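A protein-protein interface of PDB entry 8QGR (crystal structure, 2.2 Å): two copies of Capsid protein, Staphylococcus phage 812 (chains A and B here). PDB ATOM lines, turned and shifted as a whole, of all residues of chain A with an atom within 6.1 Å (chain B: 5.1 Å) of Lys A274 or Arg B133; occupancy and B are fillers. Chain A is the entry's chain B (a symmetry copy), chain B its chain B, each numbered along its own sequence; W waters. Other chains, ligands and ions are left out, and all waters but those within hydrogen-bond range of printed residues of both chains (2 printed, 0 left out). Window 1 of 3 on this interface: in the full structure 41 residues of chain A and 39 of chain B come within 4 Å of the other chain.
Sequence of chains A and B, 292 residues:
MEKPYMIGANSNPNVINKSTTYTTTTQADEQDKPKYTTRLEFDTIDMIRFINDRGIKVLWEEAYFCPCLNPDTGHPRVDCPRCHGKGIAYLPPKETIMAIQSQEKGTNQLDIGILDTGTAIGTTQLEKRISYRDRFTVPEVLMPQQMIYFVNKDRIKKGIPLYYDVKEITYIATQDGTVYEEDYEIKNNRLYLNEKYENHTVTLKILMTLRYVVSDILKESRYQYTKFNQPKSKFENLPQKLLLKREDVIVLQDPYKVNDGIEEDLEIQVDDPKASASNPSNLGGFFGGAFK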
ATOM      1  N   THR A 117     -28.192  30.978   8.174  1.00  0.00           N
ATOM      2  CA  THR A 117     -27.946  30.147   7.010  1.00  0.00           C
ATOM      3  C   THR A 117     -29.258  29.672   6.379  1.00  0.00           C
ATOM      4  O   THR A 117     -30.138  29.114   7.033  1.00  0.00           O
ATOM      5  CB  THR A 117     -26.996  28.978   7.319  1.00  0.00           C
ATOM      6  OG1 THR A 117     -26.787  28.258   6.103  1.00  0.00           O
ATOM      7  CG2 THR A 117     -27.512  28.023   8.370  1.00  0.00           C
ATOM      8  N   GLN A 145     -24.881  18.879  -2.719  1.00  0.00           N
ATOM      9  CA  GLN A 145     -24.929  18.295  -1.395  1.00  0.00           C
ATOM     10  C   GLN A 145     -24.028  17.058  -1.389  1.00  0.00           C
ATOM     11  O   GLN A 145     -23.706  16.508  -2.439  1.00  0.00           O
ATOM     12  CB  GLN A 145     -26.398  18.024  -1.055  1.00  0.00           C
ATOM     13  CG  GLN A 145     -26.647  17.544   0.364  1.00  0.00           C
ATOM     14  CD  GLN A 145     -26.063  18.439   1.431  1.00  0.00           C
ATOM     15  OE1 GLN A 145     -24.849  18.554   1.569  1.00  0.00           O
ATOM     16  NE2 GLN A 145     -26.929  19.009   2.252  1.00  0.00           N
ATOM     17  N   GLN A 146     -23.576  16.671  -0.195  1.00  0.00           N
ATOM     18  CA  GLN A 146     -22.781  15.469  -0.009  1.00  0.00           C
ATOM     19  C   GLN A 146     -23.408  14.660   1.126  1.00  0.00           C
ATOM     20  O   GLN A 146     -23.906  15.243   2.079  1.00  0.00           O
ATOM     21  CB  GLN A 146     -21.318  15.802   0.318  1.00  0.00           C
ATOM     22  CG  GLN A 146     -20.596  16.647  -0.729  1.00  0.00           C
ATOM     23  CD  GLN A 146     -20.366  18.090  -0.341  1.00  0.00           C
ATOM     24  OE1 GLN A 146     -21.217  18.747   0.258  1.00  0.00           O
ATOM     25  NE2 GLN A 146     -19.180  18.596  -0.659  1.00  0.00           N
ATOM     26  N   MET A 147     -23.342  13.326   1.050  1.00  0.00           N
ATOM     27  CA  MET A 147     -23.945  12.463   2.054  1.00  0.00           C
ATOM     28  C   MET A 147     -23.194  11.139   2.085  1.00  0.00           C
ATOM     29  O   MET A 147     -22.485  10.811   1.140  1.00  0.00           O
ATOM     30  CB  MET A 147     -25.411  12.224   1.700  1.00  0.00           C
ATOM     31  CG  MET A 147     -25.595  12.063   0.207  1.00  0.00           C
ATOM     32  SD  MET A 147     -26.776  13.247  -0.423  1.00  0.00           S
ATOM     33  CE  MET A 147     -25.691  14.523  -1.035  1.00  0.00           C
ATOM     34  N   ARG A 246     -34.019  27.646   2.922  1.00  0.00           N
ATOM     35  CA  ARG A 246     -33.450  26.793   1.890  1.00  0.00           C
ATOM     36  C   ARG A 246     -33.456  25.360   2.413  1.00  0.00           C
ATOM     37  O   ARG A 246     -33.188  25.104   3.579  1.00  0.00           O
ATOM     38  CB  ARG A 246     -32.048  27.294   1.514  1.00  0.00           C
ATOM     39  CG  ARG A 246     -31.580  26.937   0.109  1.00  0.00           C
ATOM     40  CD  ARG A 246     -30.209  27.548  -0.129  1.00  0.00           C
ATOM     41  NE  ARG A 246     -29.236  26.955   0.777  1.00  0.00           N
ATOM     42  CZ  ARG A 246     -28.121  27.539   1.205  1.00  0.00           C
ATOM     43  NH1 ARG A 246     -27.348  26.906   2.072  1.00  0.00           N
ATOM     44  NH2 ARG A 246     -27.805  28.762   0.805  1.00  0.00           N
ATOM     45  N   ASP A 248     -31.641  22.669   2.173  1.00  0.00           N
ATOM     46  CA  ASP A 248     -30.474  21.967   2.682  1.00  0.00           C
ATOM     47  C   ASP A 248     -30.216  22.308   4.148  1.00  0.00           C
ATOM     48  O   ASP A 248     -29.361  21.691   4.779  1.00  0.00           O
ATOM     49  CB  ASP A 248     -29.239  22.303   1.853  1.00  0.00           C
ATOM     50  CG  ASP A 248     -28.987  23.796   1.826  1.00  0.00           C
ATOM     51  OD1 ASP A 248     -29.739  24.493   1.130  1.00  0.00           O
ATOM     52  OD2 ASP A 248     -28.082  24.247   2.549  1.00  0.00           O
ATOM     53  N   VAL A 249     -30.940  23.293   4.688  1.00  0.00           N
ATOM     54  CA  VAL A 249     -30.766  23.658   6.081  1.00  0.00           C
ATOM     55  C   VAL A 249     -31.845  22.988   6.932  1.00  0.00           C
ATOM     56  O   VAL A 249     -31.789  23.043   8.154  1.00  0.00           O
ATOM     57  CB  VAL A 249     -30.764  25.188   6.238  1.00  0.00           C
ATOM     58  CG1 VAL A 249     -31.008  25.614   7.670  1.00  0.00           C
ATOM     59  CG2 VAL A 249     -29.480  25.792   5.698  1.00  0.00           C
ATOM     60  N   ASP A 272     -17.915  19.072  10.474  1.00  0.00           N
ATOM     61  CA  ASP A 272     -18.499  19.531   9.230  1.00  0.00           C
ATOM     62  C   ASP A 272     -18.535  21.052   9.262  1.00  0.00           C
ATOM     63  O   ASP A 272     -19.122  21.623  10.167  1.00  0.00           O
ATOM     64  CB  ASP A 272     -19.907  18.957   9.062  1.00  0.00           C
ATOM     65  CG  ASP A 272     -20.540  19.280   7.721  1.00  0.00           C
ATOM     66  OD1 ASP A 272     -19.918  20.021   6.940  1.00  0.00           O
ATOM     67  OD2 ASP A 272     -21.648  18.795   7.472  1.00  0.00           O
ATOM     68  N   PRO A 273     -17.906  21.752   8.292  1.00  0.00           N
ATOM     69  CA  PRO A 273     -17.918  23.213   8.286  1.00  0.00           C
ATOM     70  C   PRO A 273     -19.178  23.830   7.683  1.00  0.00           C
ATOM     71  O   PRO A 273     -19.317  25.046   7.647  1.00  0.00           O
ATOM     72  CB  PRO A 273     -16.690  23.536   7.429  1.00  0.00           C
ATOM     73  CG  PRO A 273     -16.650  22.399   6.420  1.00  0.00           C
ATOM     74  CD  PRO A 273     -17.138  21.182   7.175  1.00  0.00           C
ATOM     75  N   LYS A 274     -20.093  23.003   7.175  1.00  0.00           N
ATOM     76  CA  LYS A 274     -21.339  23.551   6.670  1.00  0.00           C
ATOM     77  C   LYS A 274     -22.018  24.350   7.779  1.00  0.00           C
ATOM     78  O   LYS A 274     -22.177  23.853   8.888  1.00  0.00           O
ATOM     79  CB  LYS A 274     -22.281  22.454   6.174  1.00  0.00           C
ATOM     80  CG  LYS A 274     -23.505  22.976   5.438  1.00  0.00           C
ATOM     81  CD  LYS A 274     -24.352  21.867   4.825  1.00  0.00           C
ATOM     82  CE  LYS A 274     -25.361  22.381   3.822  1.00  0.00           C
ATOM     83  NZ  LYS A 274     -26.396  23.241   4.444  1.00  0.00           N
ATOM     84  N   ALA A 275     -22.427  25.588   7.480  1.00  0.00           N
ATOM     85  CA  ALA A 275     -23.040  26.437   8.492  1.00  0.00           C
ATOM     86  C   ALA A 275     -24.297  25.760   9.054  1.00  0.00           C
ATOM     87  O   ALA A 275     -25.075  25.156   8.311  1.00  0.00           O
ATOM     88  CB  ALA A 275     -23.327  27.790   7.909  1.00  0.00           C
ATOM     89  N   SER A 276     -24.465  25.840  10.385  1.00  0.00           N
ATOM     90  CA  SER A 276     -25.595  25.233  11.084  1.00  0.00           C
ATOM     91  C   SER A 276     -26.781  26.206  11.124  1.00  0.00           C
ATOM     92  O   SER A 276     -26.774  27.069  12.023  1.00  0.00           O
ATOM     93  CB  SER A 276     -25.227  24.793  12.494  1.00  0.00           C
ATOM     94  OG  SER A 276     -24.250  23.758  12.492  1.00  0.00           O
ATOM     95  N   ALA B  63     -14.931  18.674  -2.534  1.00  0.00           N
ATOM     96  CA  ALA B  63     -14.909  17.845  -1.329  1.00  0.00           C
ATOM     97  C   ALA B  63     -16.020  16.794  -1.313  1.00  0.00           C
ATOM     98  O   ALA B  63     -17.111  17.001  -1.845  1.00  0.00           O
ATOM     99  CB  ALA B  63     -15.037  18.728  -0.110  1.00  0.00           C
ATOM    100  N   PHE B  65     -17.413  13.395   1.622  1.00  0.00           N
ATOM    101  CA  PHE B  65     -17.190  12.679   2.866  1.00  0.00           C
ATOM    102  C   PHE B  65     -16.400  11.411   2.577  1.00  0.00           C
ATOM    103  O   PHE B  65     -16.771  10.628   1.699  1.00  0.00           O
ATOM    104  CB  PHE B  65     -18.511  12.354   3.571  1.00  0.00           C
ATOM    105  CG  PHE B  65     -19.207  13.558   4.148  1.00  0.00           C
ATOM    106  CD1 PHE B  65     -18.653  14.249   5.206  1.00  0.00           C
ATOM    107  CD2 PHE B  65     -20.395  14.020   3.605  1.00  0.00           C
ATOM    108  CE1 PHE B  65     -19.285  15.364   5.733  1.00  0.00           C
ATOM    109  CE2 PHE B  65     -21.027  15.137   4.129  1.00  0.00           C
ATOM    110  CZ  PHE B  65     -20.475  15.801   5.197  1.00  0.00           C
ATOM    111  N   ILE B  88     -13.165  14.204   5.686  1.00  0.00           N
ATOM    112  CA  ILE B  88     -13.465  14.898   4.452  1.00  0.00           C
ATOM    113  C   ILE B  88     -12.261  14.776   3.524  1.00  0.00           C
ATOM    114  O   ILE B  88     -11.133  15.010   3.941  1.00  0.00           O
ATOM    115  CB  ILE B  88     -13.855  16.360   4.723  1.00  0.00           C
ATOM    116  CG1 ILE B  88     -15.126  16.421   5.578  1.00  0.00           C
ATOM    117  CG2 ILE B  88     -14.004  17.111   3.409  1.00  0.00           C
ATOM    118  CD1 ILE B  88     -15.634  17.821   5.842  1.00  0.00           C
ATOM    119  N   TYR B  90     -10.839  15.182  -0.821  1.00  0.00           N
ATOM    120  CA  TYR B  90     -10.882  16.170  -1.880  1.00  0.00           C
ATOM    121  C   TYR B  90     -10.430  15.577  -3.207  1.00  0.00           C
ATOM    122  O   TYR B  90      -9.527  14.742  -3.246  1.00  0.00           O
ATOM    123  CB  TYR B  90      -9.971  17.329  -1.489  1.00  0.00           C
ATOM    124  CG  TYR B  90     -10.337  17.943  -0.164  1.00  0.00           C
ATOM    125  CD1 TYR B  90     -11.466  18.741  -0.037  1.00  0.00           C
ATOM    126  CD2 TYR B  90      -9.597  17.676   0.973  1.00  0.00           C
ATOM    127  CE1 TYR B  90     -11.818  19.300   1.180  1.00  0.00           C
ATOM    128  CE2 TYR B  90      -9.945  18.209   2.203  1.00  0.00           C
ATOM    129  CZ  TYR B  90     -11.059  19.025   2.302  1.00  0.00           C
ATOM    130  OH  TYR B  90     -11.434  19.556   3.501  1.00  0.00           O
ATOM    131  N   SER B 131     -19.527  23.721  -3.683  1.00  0.00           N
ATOM    132  CA  SER B 131     -20.310  23.158  -2.597  1.00  0.00           C
ATOM    133  C   SER B 131     -19.677  23.454  -1.240  1.00  0.00           C
ATOM    134  O   SER B 131     -18.503  23.834  -1.150  1.00  0.00           O
ATOM    135  CB  SER B 131     -20.464  21.654  -2.769  1.00  0.00           C
ATOM    136  OG  SER B 131     -21.373  21.112  -1.807  1.00  0.00           O
ATOM    137  N   TYR B 132     -20.504  23.236  -0.204  1.00  0.00           N
ATOM    138  CA  TYR B 132     -20.104  23.242   1.188  1.00  0.00           C
ATOM    139  C   TYR B 132     -18.946  22.263   1.322  1.00  0.00           C
ATOM    140  O   TYR B 132     -18.959  21.238   0.647  1.00  0.00           O
ATOM    141  CB  TYR B 132     -21.276  22.771   2.061  1.00  0.00           C
ATOM    142  CG  TYR B 132     -22.621  23.280   1.603  1.00  0.00           C
ATOM    143  CD1 TYR B 132     -22.996  24.594   1.808  1.00  0.00           C
ATOM    144  CD2 TYR B 132     -23.466  22.473   0.858  1.00  0.00           C
ATOM    145  CE1 TYR B 132     -24.211  25.074   1.346  1.00  0.00           C
ATOM    146  CE2 TYR B 132     -24.684  22.933   0.388  1.00  0.00           C
ATOM    147  CZ  TYR B 132     -25.053  24.244   0.626  1.00  0.00           C
ATOM    148  OH  TYR B 132     -26.245  24.715   0.157  1.00  0.00           O
ATOM    149  N   ARG B 133     -17.955  22.606   2.157  1.00  0.00           N
ATOM    150  CA  ARG B 133     -16.844  21.723   2.490  1.00  0.00           C
ATOM    151  C   ARG B 133     -15.723  21.770   1.444  1.00  0.00           C
ATOM    152  O   ARG B 133     -14.611  21.336   1.747  1.00  0.00           O
ATOM    153  CB  ARG B 133     -17.353  20.296   2.639  1.00  0.00           C
ATOM    154  CG  ARG B 133     -18.396  20.153   3.736  1.00  0.00           C
ATOM    155  CD  ARG B 133     -19.542  19.300   3.237  1.00  0.00           C
ATOM    156  NE  ARG B 133     -20.580  19.244   4.242  1.00  0.00           N
ATOM    157  CZ  ARG B 133     -21.860  18.993   4.007  1.00  0.00           C
ATOM    158  NH1 ARG B 133     -22.705  19.001   5.016  1.00  0.00           N
ATOM    159  NH2 ARG B 133     -22.295  18.773   2.774  1.00  0.00           N
ATOM    160  N   ASP B 134     -16.007  22.235   0.218  1.00  0.00           N
ATOM    161  CA  ASP B 134     -14.950  22.370  -0.775  1.00  0.00           C
ATOM    162  C   ASP B 134     -13.863  23.299  -0.221  1.00  0.00           C
ATOM    163  O   ASP B 134     -14.141  24.164   0.615  1.00  0.00           O
ATOM    164  CB  ASP B 134     -15.442  22.938  -2.104  1.00  0.00           C
ATOM    165  CG  ASP B 134     -16.409  22.068  -2.889  1.00  0.00           C
ATOM    166  OD1 ASP B 134     -16.668  20.925  -2.463  1.00  0.00           O
ATOM    167  OD2 ASP B 134     -16.893  22.550  -3.938  1.00  0.00           O
ATOM    168  N   ARG B 135     -12.625  23.138  -0.714  1.00  0.00           N
ATOM    169  CA  ARG B 135     -11.497  23.869  -0.158  1.00  0.00           C
ATOM    170  C   ARG B 135     -10.839  24.726  -1.232  1.00  0.00           C
ATOM    171  O   ARG B 135     -10.633  24.266  -2.349  1.00  0.00           O
ATOM    172  CB  ARG B 135     -10.495  22.898   0.479  1.00  0.00           C
ATOM    173  CG  ARG B 135      -9.267  23.564   1.091  1.00  0.00           C
ATOM    174  CD  ARG B 135      -8.424  22.553   1.849  1.00  0.00           C
ATOM    175  NE  ARG B 135      -7.886  21.486   1.007  1.00  0.00           N
ATOM    176  CZ  ARG B 135      -7.268  20.398   1.463  1.00  0.00           C
ATOM    177  NH1 ARG B 135      -6.685  19.564   0.619  1.00  0.00           N
ATOM    178  NH2 ARG B 135      -7.191  20.167   2.762  1.00  0.00           N
ATOM    179  N   VAL B 213     -12.291  26.659   3.691  1.00  0.00           N
ATOM    180  CA  VAL B 213     -13.310  25.703   3.298  1.00  0.00           C
ATOM    181  C   VAL B 213     -14.651  26.437   3.277  1.00  0.00           C
ATOM    182  O   VAL B 213     -14.839  27.412   4.005  1.00  0.00           O
ATOM    183  CB  VAL B 213     -13.320  24.456   4.198  1.00  0.00           C
ATOM    184  CG1 VAL B 213     -11.987  23.722   4.162  1.00  0.00           C
ATOM    185  CG2 VAL B 213     -13.727  24.777   5.625  1.00  0.00           C
ATOM    186  N   VAL B 214     -15.559  25.984   2.401  1.00  0.00           N
ATOM    187  CA  VAL B 214     -16.848  26.626   2.207  1.00  0.00           C
ATOM    188  C   VAL B 214     -17.782  26.234   3.346  1.00  0.00           C
ATOM    189  O   VAL B 214     -18.019  25.050   3.578  1.00  0.00           O
ATOM    190  CB  VAL B 214     -17.463  26.232   0.853  1.00  0.00           C
ATOM    191  CG1 VAL B 214     -18.837  26.862   0.667  1.00  0.00           C
ATOM    192  CG2 VAL B 214     -16.541  26.569  -0.307  1.00  0.00           C
ATOM    193  N   SER B 215     -18.317  27.229   4.058  1.00  0.00           N
ATOM    194  CA  SER B 215     -19.319  26.935   5.069  1.00  0.00           C
ATOM    195  C   SER B 215     -20.710  27.150   4.485  1.00  0.00           C
ATOM    196  O   SER B 215     -21.663  26.518   4.934  1.00  0.00           O
ATOM    197  CB  SER B 215     -19.148  27.723   6.347  1.00  0.00           C
ATOM    198  OG  SER B 215     -19.365  29.096   6.123  1.00  0.00           O
HETATM  199  O   HOH W   1     -19.855  12.809   0.000  1.00  0.00           O
HETATM  200  O   HOH W   2     -25.490  18.209   5.054  1.00  0.00           O
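Water W2 lies within hydrogen-bond range of the guanidinium group (NH1) of Arg B133 and the side-chain amide nitrogen (NE2) of Gln A145. Water W1 lies within hydrogen-bond range of N of Phe B65 (3.0 Å) and O of Met A147 (3.5 Å).
The side-chain amide nitrogen of Gln A146 sits at hydrogen-bond distance from the backbone carbonyl oxygen of Ala B63 (2.9 Å). The guanidinium group of Arg B133 sits at hydrogen-bond distance from the side-chain amide oxygen of Gln A146 (2.7 Å). The guanidinium group (NH1) of Arg B133 lies within salt-bridge range of the side-chain carboxylate (OD2) of Asp A272 (2.7 Å). O of Ser B215 lies within hydrogen-bond range of N of Ala A275 (2.8 Å). The side-chain hydroxyl (OG) of Ser B131 sits at hydrogen-bond distance from the side-chain amide oxygen (OE1) of Gln A146. The guanidinium group of Arg B133 sits at hydrogen-bond distance from the side-chain amide oxygen of Gln A145 (2.8 Å). The side-chain amide nitrogen (NE2) of Gln A146 is in hydrogen-bond range of the backbone carbonyl oxygen (O) of Tyr B132, 3.0 Å away. The side-chain hydroxyl of Tyr B132 lies within hydrogen-bond range of the side-chain carboxylate of Asp A248 (3.1 Å). OH of Tyr B132 lies within hydrogen-bond range of NH1 of Arg A246 (3.1 Å).
Among the printed residues, merely in contact across the chains: Pro A273 with Ser B215, Lys A274 with Arg B133, Lys A274 with Ser B215, Lys A274 with Tyr B132, Gln A146 with Phe B65, Pro A273 with Val B213, Pro A273 with Arg B133, Gln A146 with Asp B134, Pro A273 with Ile B88, Asp A272 with Phe B65 and Met A147 with Phe B65.
Printed residues of chain A that touch a printed residue of chain B: Gln A145, Gln A146, Met A147, Arg A246, Asp A248, Asp A272, Pro A273, Lys A274 and Ala A275. Along chain A the printed residues that touch a printed residue of chain B span positions 145 to 275. Among the printed residues, 20 pairs touch across the chains. Among the printed residues, Asp or Glu carboxylates within 4 Å of a Lys or Arg side-chain nitrogen of the other chain: Asp A272 with Arg B133.
Of chain B, only Tyr B132, Arg B133 and Ser B215 come within 4 Å of Lys A274. Arg B133 touches five residues of chain A. Printed residues of chain A within 4 Å of Tyr B132: Gln A146, Arg A246, Asp A248 and Lys A274. Of the printed residues of chain B, Pro A273 touches Ile B88 (3.9 Å), Arg B133 (3.8 Å), Val B213 (3.7 Å) and Ser B215 (3.0 Å). Arg B135 touches none of the printed residues of chain A. Val B214 touches none of the printed residues of chain A. The nearest residue of chain B that does not touch Lys A274 is Val B214 (4.6 Å). The nearest printed residue of chain A that does not touch Ser B215 is Thr A117 (5.5 Å).
No position is printed for both chains.
The backbone NH (N) of Val B214 lies within hydrogen-bond range of the backbone carbonyl oxygen (O) of Asp B134, at 2.9 Å. The side-chain carboxylate of Asp A248 lies within salt-bridge range of the guanidinium group of Arg A246 (2.5 Å). OD2 of Asp A248 lies within salt-bridge range of NZ of Lys A274 (2.7 Å). The backbone NH (N) of Lys A274 is in hydrogen-bond range of the side-chain carboxylate (OD1) of Asp A272, 3.0 Å away. The backbone NH (N) of Arg B133 lies within hydrogen-bond range of the backbone carbonyl oxygen (O) of Val B214 (2.8 Å). The side-chain carboxylate (OD2) of Asp B134 lies within hydrogen-bond range of the backbone NH (N) of Ser B131, at 2.9 Å.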
